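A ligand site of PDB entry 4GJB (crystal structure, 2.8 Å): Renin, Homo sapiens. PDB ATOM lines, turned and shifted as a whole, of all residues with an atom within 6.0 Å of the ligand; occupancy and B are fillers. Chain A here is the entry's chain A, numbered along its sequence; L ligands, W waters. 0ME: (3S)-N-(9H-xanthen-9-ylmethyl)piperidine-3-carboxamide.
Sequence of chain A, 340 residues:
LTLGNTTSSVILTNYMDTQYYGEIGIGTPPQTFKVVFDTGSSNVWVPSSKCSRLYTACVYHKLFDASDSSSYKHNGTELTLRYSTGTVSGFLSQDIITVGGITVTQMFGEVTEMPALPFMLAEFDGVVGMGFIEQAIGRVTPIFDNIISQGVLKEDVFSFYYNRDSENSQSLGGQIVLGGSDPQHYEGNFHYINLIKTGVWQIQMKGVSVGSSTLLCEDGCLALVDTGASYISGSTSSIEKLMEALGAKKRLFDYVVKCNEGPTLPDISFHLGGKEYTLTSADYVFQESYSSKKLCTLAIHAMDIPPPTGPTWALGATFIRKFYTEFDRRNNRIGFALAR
N of Ser 84 lies within hydrogen-bond range of O18 of the ligand, at 3.1 Å. OG of Ser 84 is in hydrogen-bond range of O18 of the ligand, at 2.7 Å. The side-chain carboxylate (OD1) of Asp 38 lies within salt-bridge range of a nitrogen (N23) of the ligand (2.7 Å). A nitrogen (N16) of the ligand sits at hydrogen-bond distance from the backbone carbonyl oxygen (O) of Gly 228. The side-chain carboxylate (OD2) of Asp 226 is in salt-bridge range of a nitrogen (N23) of the ligand (3.2 Å).
The side-chain carboxylate (OD1) of Asp 38 lies close to the side-chain carboxylate (OD1) of Asp 226 (2.7 Å). The side-chain carboxylate of Asp 38 lies within hydrogen-bond range of the backbone NH of Gly 40 (2.9 Å). The side-chain hydroxyl of Ser 41 sits at hydrogen-bond distance from the side-chain carboxylate of Asp 38, 2.6 Å away. The backbone NH (N) of Gly 228 sits close to the side-chain carboxylate (OD1) of Asp 226, at 3.1 Å. The backbone NH of Gly 40 is in hydrogen-bond range of the side-chain carboxylate of Asp 226. The backbone carbonyl oxygen (O) of Val 127 lies within hydrogen-bond range of the backbone NH (N) of Trp 45, 2.9 Å away. OH of Tyr 83 sits at hydrogen-bond distance from NE1 of Trp 45. The backbone carbonyl oxygen (O) of Leu 121 lies within hydrogen-bond range of the side-chain amide nitrogen (NE2) of Gln 19 (3.2 Å).
Merely in contact with the ligand: Gln 19 (3.6 Å), Gly 40 (3.6 Å), Tyr 83 (3.4 Å), Thr 85 (3.9 Å), Pro 118 (3.8 Å), Phe 119 (3.8 Å), Phe 124 (3.7 Å) and Val 127 (3.3 Å).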
ATOM      1  N   THR A  18      29.237  -0.667   4.377  1.00  0.00           N
ATOM      2  CA  THR A  18      28.062  -0.551   3.502  1.00  0.00           C
ATOM      3  C   THR A  18      26.974   0.332   4.082  1.00  0.00           C
ATOM      4  O   THR A  18      26.165   0.879   3.333  1.00  0.00           O
ATOM      5  CB  THR A  18      27.513  -1.925   3.083  1.00  0.00           C
ATOM      6  OG1 THR A  18      27.053  -2.619   4.229  1.00  0.00           O
ATOM      7  CG2 THR A  18      28.513  -2.749   2.301  1.00  0.00           C
ATOM      8  N   GLN A  19      26.916   0.436   5.429  1.00  0.00           N
ATOM      9  CA  GLN A  19      25.917   1.207   6.145  1.00  0.00           C
ATOM     10  C   GLN A  19      26.546   2.057   7.230  1.00  0.00           C
ATOM     11  O   GLN A  19      27.245   1.549   8.116  1.00  0.00           O
ATOM     12  CB  GLN A  19      24.878   0.272   6.738  1.00  0.00           C
ATOM     13  CG  GLN A  19      24.046  -0.463   5.674  1.00  0.00           C
ATOM     14  CD  GLN A  19      23.060  -1.432   6.253  1.00  0.00           C
ATOM     15  OE1 GLN A  19      22.366  -1.148   7.238  1.00  0.00           O
ATOM     16  NE2 GLN A  19      22.967  -2.591   5.623  1.00  0.00           N
ATOM     17  N   VAL A  36      20.103   6.789   8.374  1.00  0.00           N
ATOM     18  CA  VAL A  36      21.089   6.945   7.324  1.00  0.00           C
ATOM     19  C   VAL A  36      20.828   8.350   6.803  1.00  0.00           C
ATOM     20  O   VAL A  36      19.652   8.712   6.604  1.00  0.00           O
ATOM     21  CB  VAL A  36      20.915   5.846   6.246  1.00  0.00           C
ATOM     22  CG1 VAL A  36      21.055   6.376   4.832  1.00  0.00           C
ATOM     23  CG2 VAL A  36      21.902   4.722   6.498  1.00  0.00           C
ATOM     24  N   ASP A  38      21.132  10.608   3.829  1.00  0.00           N
ATOM     25  CA  ASP A  38      21.203  10.384   2.401  1.00  0.00           C
ATOM     26  C   ASP A  38      21.041  11.637   1.568  1.00  0.00           C
ATOM     27  O   ASP A  38      19.955  12.185   1.500  1.00  0.00           O
ATOM     28  CB  ASP A  38      20.135   9.304   2.050  1.00  0.00           C
ATOM     29  CG  ASP A  38      19.880   9.026   0.587  1.00  0.00           C
ATOM     30  OD1 ASP A  38      20.813   9.121  -0.218  1.00  0.00           O
ATOM     31  OD2 ASP A  38      18.754   8.630   0.254  1.00  0.00           O
ATOM     32  N   THR A  39      22.107  12.038   0.862  1.00  0.00           N
ATOM     33  CA  THR A  39      22.104  13.198  -0.040  1.00  0.00           C
ATOM     34  C   THR A  39      21.389  12.906  -1.373  1.00  0.00           C
ATOM     35  O   THR A  39      21.124  13.834  -2.155  1.00  0.00           O
ATOM     36  CB  THR A  39      23.508  13.738  -0.294  1.00  0.00           C
ATOM     37  OG1 THR A  39      24.313  12.686  -0.820  1.00  0.00           O
ATOM     38  CG2 THR A  39      24.146  14.312   0.940  1.00  0.00           C
ATOM     39  N   GLY A  40      21.073  11.639  -1.623  1.00  0.00           N
ATOM     40  CA  GLY A  40      20.381  11.166  -2.811  1.00  0.00           C
ATOM     41  C   GLY A  40      18.877  11.291  -2.764  1.00  0.00           C
ATOM     42  O   GLY A  40      18.229  11.124  -3.806  1.00  0.00           O
ATOM     43  N   SER A  41      18.287  11.563  -1.565  1.00  0.00           N
ATOM     44  CA  SER A  41      16.848  11.752  -1.324  1.00  0.00           C
ATOM     45  C   SER A  41      16.594  12.941  -0.380  1.00  0.00           C
ATOM     46  O   SER A  41      17.552  13.460   0.203  1.00  0.00           O
ATOM     47  CB  SER A  41      16.183  10.457  -0.836  1.00  0.00           C
ATOM     48  OG  SER A  41      16.545  10.046   0.470  1.00  0.00           O
ATOM     49  N   TRP A  45      11.929   9.824   7.263  1.00  0.00           N
ATOM     50  CA  TRP A  45      10.972   8.742   7.595  1.00  0.00           C
ATOM     51  C   TRP A  45      11.537   7.767   8.605  1.00  0.00           C
ATOM     52  O   TRP A  45      12.705   7.429   8.539  1.00  0.00           O
ATOM     53  CB  TRP A  45      10.434   7.966   6.350  1.00  0.00           C
ATOM     54  CG  TRP A  45      11.422   7.088   5.621  1.00  0.00           C
ATOM     55  CD1 TRP A  45      12.057   7.394   4.448  1.00  0.00           C
ATOM     56  CD2 TRP A  45      11.787   5.737   5.926  1.00  0.00           C
ATOM     57  NE1 TRP A  45      12.827   6.339   4.043  1.00  0.00           N
ATOM     58  CE2 TRP A  45      12.681   5.305   4.927  1.00  0.00           C
ATOM     59  CE3 TRP A  45      11.459   4.845   6.962  1.00  0.00           C
ATOM     60  CZ2 TRP A  45      13.260   4.024   4.931  1.00  0.00           C
ATOM     61  CZ3 TRP A  45      12.050   3.587   6.980  1.00  0.00           C
ATOM     62  CH2 TRP A  45      12.929   3.178   5.964  1.00  0.00           C
ATOM     63  N   ARG A  82      10.242   5.640  -2.939  1.00  0.00           N
ATOM     64  CA  ARG A  82      10.974   4.607  -3.697  1.00  0.00           C
ATOM     65  C   ARG A  82      12.472   4.816  -3.784  1.00  0.00           C
ATOM     66  O   ARG A  82      12.907   5.853  -4.281  1.00  0.00           O
ATOM     67  CB  ARG A  82      10.330   4.302  -5.074  1.00  0.00           C
ATOM     68  CG  ARG A  82      10.012   5.507  -5.971  1.00  0.00           C
ATOM     69  CD  ARG A  82       9.694   5.065  -7.405  1.00  0.00           C
ATOM     70  NE  ARG A  82       8.674   5.907  -8.037  1.00  0.00           N
ATOM     71  CZ  ARG A  82       8.793   6.465  -9.248  1.00  0.00           C
ATOM     72  NH1 ARG A  82       7.805   7.207  -9.744  1.00  0.00           N
ATOM     73  NH2 ARG A  82       9.894   6.294  -9.960  1.00  0.00           N
ATOM     74  N   TYR A  83      13.253   3.786  -3.334  1.00  0.00           N
ATOM     75  CA  TYR A  83      14.727   3.709  -3.334  1.00  0.00           C
ATOM     76  C   TYR A  83      15.225   2.693  -4.369  1.00  0.00           C
ATOM     77  O   TYR A  83      14.442   2.252  -5.209  1.00  0.00           O
ATOM     78  CB  TYR A  83      15.254   3.443  -1.911  1.00  0.00           C
ATOM     79  CG  TYR A  83      14.782   4.506  -0.943  1.00  0.00           C
ATOM     80  CD1 TYR A  83      15.239   5.824  -1.039  1.00  0.00           C
ATOM     81  CD2 TYR A  83      13.769   4.233  -0.012  1.00  0.00           C
ATOM     82  CE1 TYR A  83      14.741   6.815  -0.216  1.00  0.00           C
ATOM     83  CE2 TYR A  83      13.279   5.232   0.821  1.00  0.00           C
ATOM     84  CZ  TYR A  83      13.773   6.524   0.727  1.00  0.00           C
ATOM     85  OH  TYR A  83      13.286   7.525   1.525  1.00  0.00           O
ATOM     86  N   SER A  84      16.501   2.345  -4.351  1.00  0.00           N
ATOM     87  CA  SER A  84      17.011   1.424  -5.354  1.00  0.00           C
ATOM     88  C   SER A  84      16.707  -0.046  -5.129  1.00  0.00           C
ATOM     89  O   SER A  84      16.380  -0.760  -6.079  1.00  0.00           O
ATOM     90  CB  SER A  84      18.491   1.654  -5.611  1.00  0.00           C
ATOM     91  OG  SER A  84      19.256   1.677  -4.418  1.00  0.00           O
ATOM     92  N   THR A  85      16.769  -0.485  -3.866  1.00  0.00           N
ATOM     93  CA  THR A  85      16.507  -1.880  -3.459  1.00  0.00           C
ATOM     94  C   THR A  85      15.026  -2.154  -3.177  1.00  0.00           C
ATOM     95  O   THR A  85      14.557  -3.249  -3.426  1.00  0.00           O
ATOM     96  CB  THR A  85      17.373  -2.294  -2.249  1.00  0.00           C
ATOM     97  OG1 THR A  85      18.056  -1.170  -1.662  1.00  0.00           O
ATOM     98  CG2 THR A  85      18.362  -3.375  -2.578  1.00  0.00           C
ATOM     99  N   GLY A  86      14.319  -1.158  -2.639  1.00  0.00           N
ATOM    100  CA  GLY A  86      12.907  -1.326  -2.304  1.00  0.00           C
ATOM    101  C   GLY A  86      12.168  -0.033  -2.028  1.00  0.00           C
ATOM    102  O   GLY A  86      12.777   1.037  -1.939  1.00  0.00           O
ATOM    103  N   PRO A 118      14.410  -4.997   1.029  1.00  0.00           N
ATOM    104  CA  PRO A 118      15.740  -5.084   1.671  1.00  0.00           C
ATOM    105  C   PRO A 118      15.857  -4.734   3.161  1.00  0.00           C
ATOM    106  O   PRO A 118      16.951  -4.886   3.739  1.00  0.00           O
ATOM    107  CB  PRO A 118      16.527  -4.031   0.893  1.00  0.00           C
ATOM    108  CG  PRO A 118      15.507  -2.946   0.666  1.00  0.00           C
ATOM    109  CD  PRO A 118      14.197  -3.660   0.442  1.00  0.00           C
ATOM    110  N   PHE A 119      14.767  -4.259   3.761  1.00  0.00           N
ATOM    111  CA  PHE A 119      14.753  -3.727   5.124  1.00  0.00           C
ATOM    112  C   PHE A 119      15.122  -4.624   6.284  1.00  0.00           C
ATOM    113  O   PHE A 119      15.511  -4.085   7.315  1.00  0.00           O
ATOM    114  CB  PHE A 119      13.544  -2.792   5.369  1.00  0.00           C
ATOM    115  CG  PHE A 119      13.488  -1.684   4.328  1.00  0.00           C
ATOM    116  CD1 PHE A 119      14.331  -0.584   4.405  1.00  0.00           C
ATOM    117  CD2 PHE A 119      12.656  -1.800   3.218  1.00  0.00           C
ATOM    118  CE1 PHE A 119      14.302   0.403   3.429  1.00  0.00           C
ATOM    119  CE2 PHE A 119      12.655  -0.830   2.224  1.00  0.00           C
ATOM    120  CZ  PHE A 119      13.472   0.267   2.342  1.00  0.00           C
ATOM    121  N   LEU A 121      17.773  -6.397   6.098  1.00  0.00           N
ATOM    122  CA  LEU A 121      19.221  -6.274   5.929  1.00  0.00           C
ATOM    123  C   LEU A 121      19.743  -4.932   6.478  1.00  0.00           C
ATOM    124  O   LEU A 121      20.923  -4.810   6.816  1.00  0.00           O
ATOM    125  CB  LEU A 121      19.595  -6.449   4.461  1.00  0.00           C
ATOM    126  CG  LEU A 121      19.059  -7.727   3.790  1.00  0.00           C
ATOM    127  CD1 LEU A 121      19.009  -7.571   2.301  1.00  0.00           C
ATOM    128  CD2 LEU A 121      19.905  -8.912   4.144  1.00  0.00           C
ATOM    129  N   ALA A 122      18.836  -3.951   6.602  1.00  0.00           N
ATOM    130  CA  ALA A 122      19.112  -2.620   7.137  1.00  0.00           C
ATOM    131  C   ALA A 122      19.354  -2.682   8.636  1.00  0.00           C
ATOM    132  O   ALA A 122      18.591  -3.315   9.369  1.00  0.00           O
ATOM    133  CB  ALA A 122      17.939  -1.697   6.818  1.00  0.00           C
ATOM    134  N   PHE A 124      19.815   0.226  10.262  1.00  0.00           N
ATOM    135  CA  PHE A 124      19.234   1.521  10.605  1.00  0.00           C
ATOM    136  C   PHE A 124      17.714   1.379  10.634  1.00  0.00           C
ATOM    137  O   PHE A 124      17.176   0.519   9.960  1.00  0.00           O
ATOM    138  CB  PHE A 124      19.685   2.572   9.571  1.00  0.00           C
ATOM    139  CG  PHE A 124      19.424   2.237   8.115  1.00  0.00           C
ATOM    140  CD1 PHE A 124      20.408   1.618   7.342  1.00  0.00           C
ATOM    141  CD2 PHE A 124      18.224   2.590   7.511  1.00  0.00           C
ATOM    142  CE1 PHE A 124      20.194   1.371   5.991  1.00  0.00           C
ATOM    143  CE2 PHE A 124      17.993   2.292   6.161  1.00  0.00           C
ATOM    144  CZ  PHE A 124      18.985   1.710   5.405  1.00  0.00           C
ATOM    145  N   VAL A 127      15.509   6.998   7.557  1.00  0.00           N
ATOM    146  CA  VAL A 127      16.287   7.778   6.614  1.00  0.00           C
ATOM    147  C   VAL A 127      16.004   9.273   6.794  1.00  0.00           C
ATOM    148  O   VAL A 127      14.839   9.672   6.860  1.00  0.00           O
ATOM    149  CB  VAL A 127      15.948   7.314   5.151  1.00  0.00           C
ATOM    150  CG1 VAL A 127      16.574   8.234   4.098  1.00  0.00           C
ATOM    151  CG2 VAL A 127      16.349   5.870   4.916  1.00  0.00           C
ATOM    152  N   ASP A 226      26.251  10.655  -3.638  1.00  0.00           N
ATOM    153  CA  ASP A 226      25.264   9.936  -2.834  1.00  0.00           C
ATOM    154  C   ASP A 226      25.759   9.244  -1.544  1.00  0.00           C
ATOM    155  O   ASP A 226      26.199   8.079  -1.537  1.00  0.00           O
ATOM    156  CB  ASP A 226      24.446   8.981  -3.757  1.00  0.00           C
ATOM    157  CG  ASP A 226      23.156   8.428  -3.180  1.00  0.00           C
ATOM    158  OD1 ASP A 226      22.730   8.909  -2.103  1.00  0.00           O
ATOM    159  OD2 ASP A 226      22.567   7.499  -3.793  1.00  0.00           O
ATOM    160  N   GLY A 228      23.977   8.003   0.619  1.00  0.00           N
ATOM    161  CA  GLY A 228      23.036   6.906   0.845  1.00  0.00           C
ATOM    162  C   GLY A 228      23.308   5.621   0.068  1.00  0.00           C
ATOM    163  O   GLY A 228      22.650   4.596   0.296  1.00  0.00           O
ATOM    164  N   ALA A 229      24.267   5.682  -0.875  1.00  0.00           N
ATOM    165  CA  ALA A 229      24.735   4.576  -1.701  1.00  0.00           C
ATOM    166  C   ALA A 229      25.941   3.947  -1.020  1.00  0.00           C
ATOM    167  O   ALA A 229      26.788   4.655  -0.481  1.00  0.00           O
ATOM    168  CB  ALA A 229      25.126   5.115  -3.051  1.00  0.00           C
ATOM    169  N   SER A 230      26.039   2.640  -1.051  1.00  0.00           N
ATOM    170  CA  SER A 230      27.150   1.929  -0.433  1.00  0.00           C
ATOM    171  C   SER A 230      28.358   1.870  -1.345  1.00  0.00           C
ATOM    172  O   SER A 230      29.503   1.845  -0.885  1.00  0.00           O
ATOM    173  CB  SER A 230      26.722   0.506  -0.055  1.00  0.00           C
ATOM    174  OG  SER A 230      25.626   0.464   0.851  1.00  0.00           O
HETATM  175  C1  0ME L   1      19.183   2.801   1.565  1.00  0.00           C
HETATM  176  C2  0ME L   1      17.869   2.262   1.677  1.00  0.00           C
HETATM  177  O3  0ME L   1      17.623   0.881   1.642  1.00  0.00           O
HETATM  178  C4  0ME L   1      20.376   1.856   1.309  1.00  0.00           C
HETATM  179  C5  0ME L   1      18.296   5.023   1.861  1.00  0.00           C
HETATM  180  C6  0ME L   1      16.993   4.497   1.933  1.00  0.00           C
HETATM  181  C7  0ME L   1      16.773   3.107   1.875  1.00  0.00           C
HETATM  182  C8  0ME L   1      19.401   4.181   1.664  1.00  0.00           C
HETATM  183  C9  0ME L   1      20.049   0.497   1.926  1.00  0.00           C
HETATM  184  C10 0ME L   1      18.689   0.074   2.066  1.00  0.00           C
HETATM  185  C11 0ME L   1      18.388  -1.176   2.639  1.00  0.00           C
HETATM  186  C12 0ME L   1      19.434  -1.995   3.088  1.00  0.00           C
HETATM  187  C13 0ME L   1      20.789  -1.588   2.944  1.00  0.00           C
HETATM  188  C14 0ME L   1      21.101  -0.344   2.377  1.00  0.00           C
HETATM  189  C15 0ME L   1      20.569   1.691  -0.237  1.00  0.00           C
HETATM  190  N16 0ME L   1      20.558   2.970  -0.984  1.00  0.00           N
HETATM  191  C17 0ME L   1      19.571   3.434  -1.807  1.00  0.00           C
HETATM  192  O18 0ME L   1      18.544   2.795  -2.044  1.00  0.00           O
HETATM  193  C19 0ME L   1      19.757   4.790  -2.460  1.00  0.00           C
HETATM  194  C20 0ME L   1      18.613   5.144  -3.464  1.00  0.00           C
HETATM  195  C21 0ME L   1      18.718   6.584  -4.070  1.00  0.00           C
HETATM  196  C22 0ME L   1      18.862   7.667  -2.968  1.00  0.00           C
HETATM  197  N23 0ME L   1      19.950   7.286  -2.047  1.00  0.00           N
HETATM  198  C24 0ME L   1      19.838   5.938  -1.425  1.00  0.00           C
HETATM  199  O   HOH W   1      23.541  -1.470   0.164  1.00  0.00           O
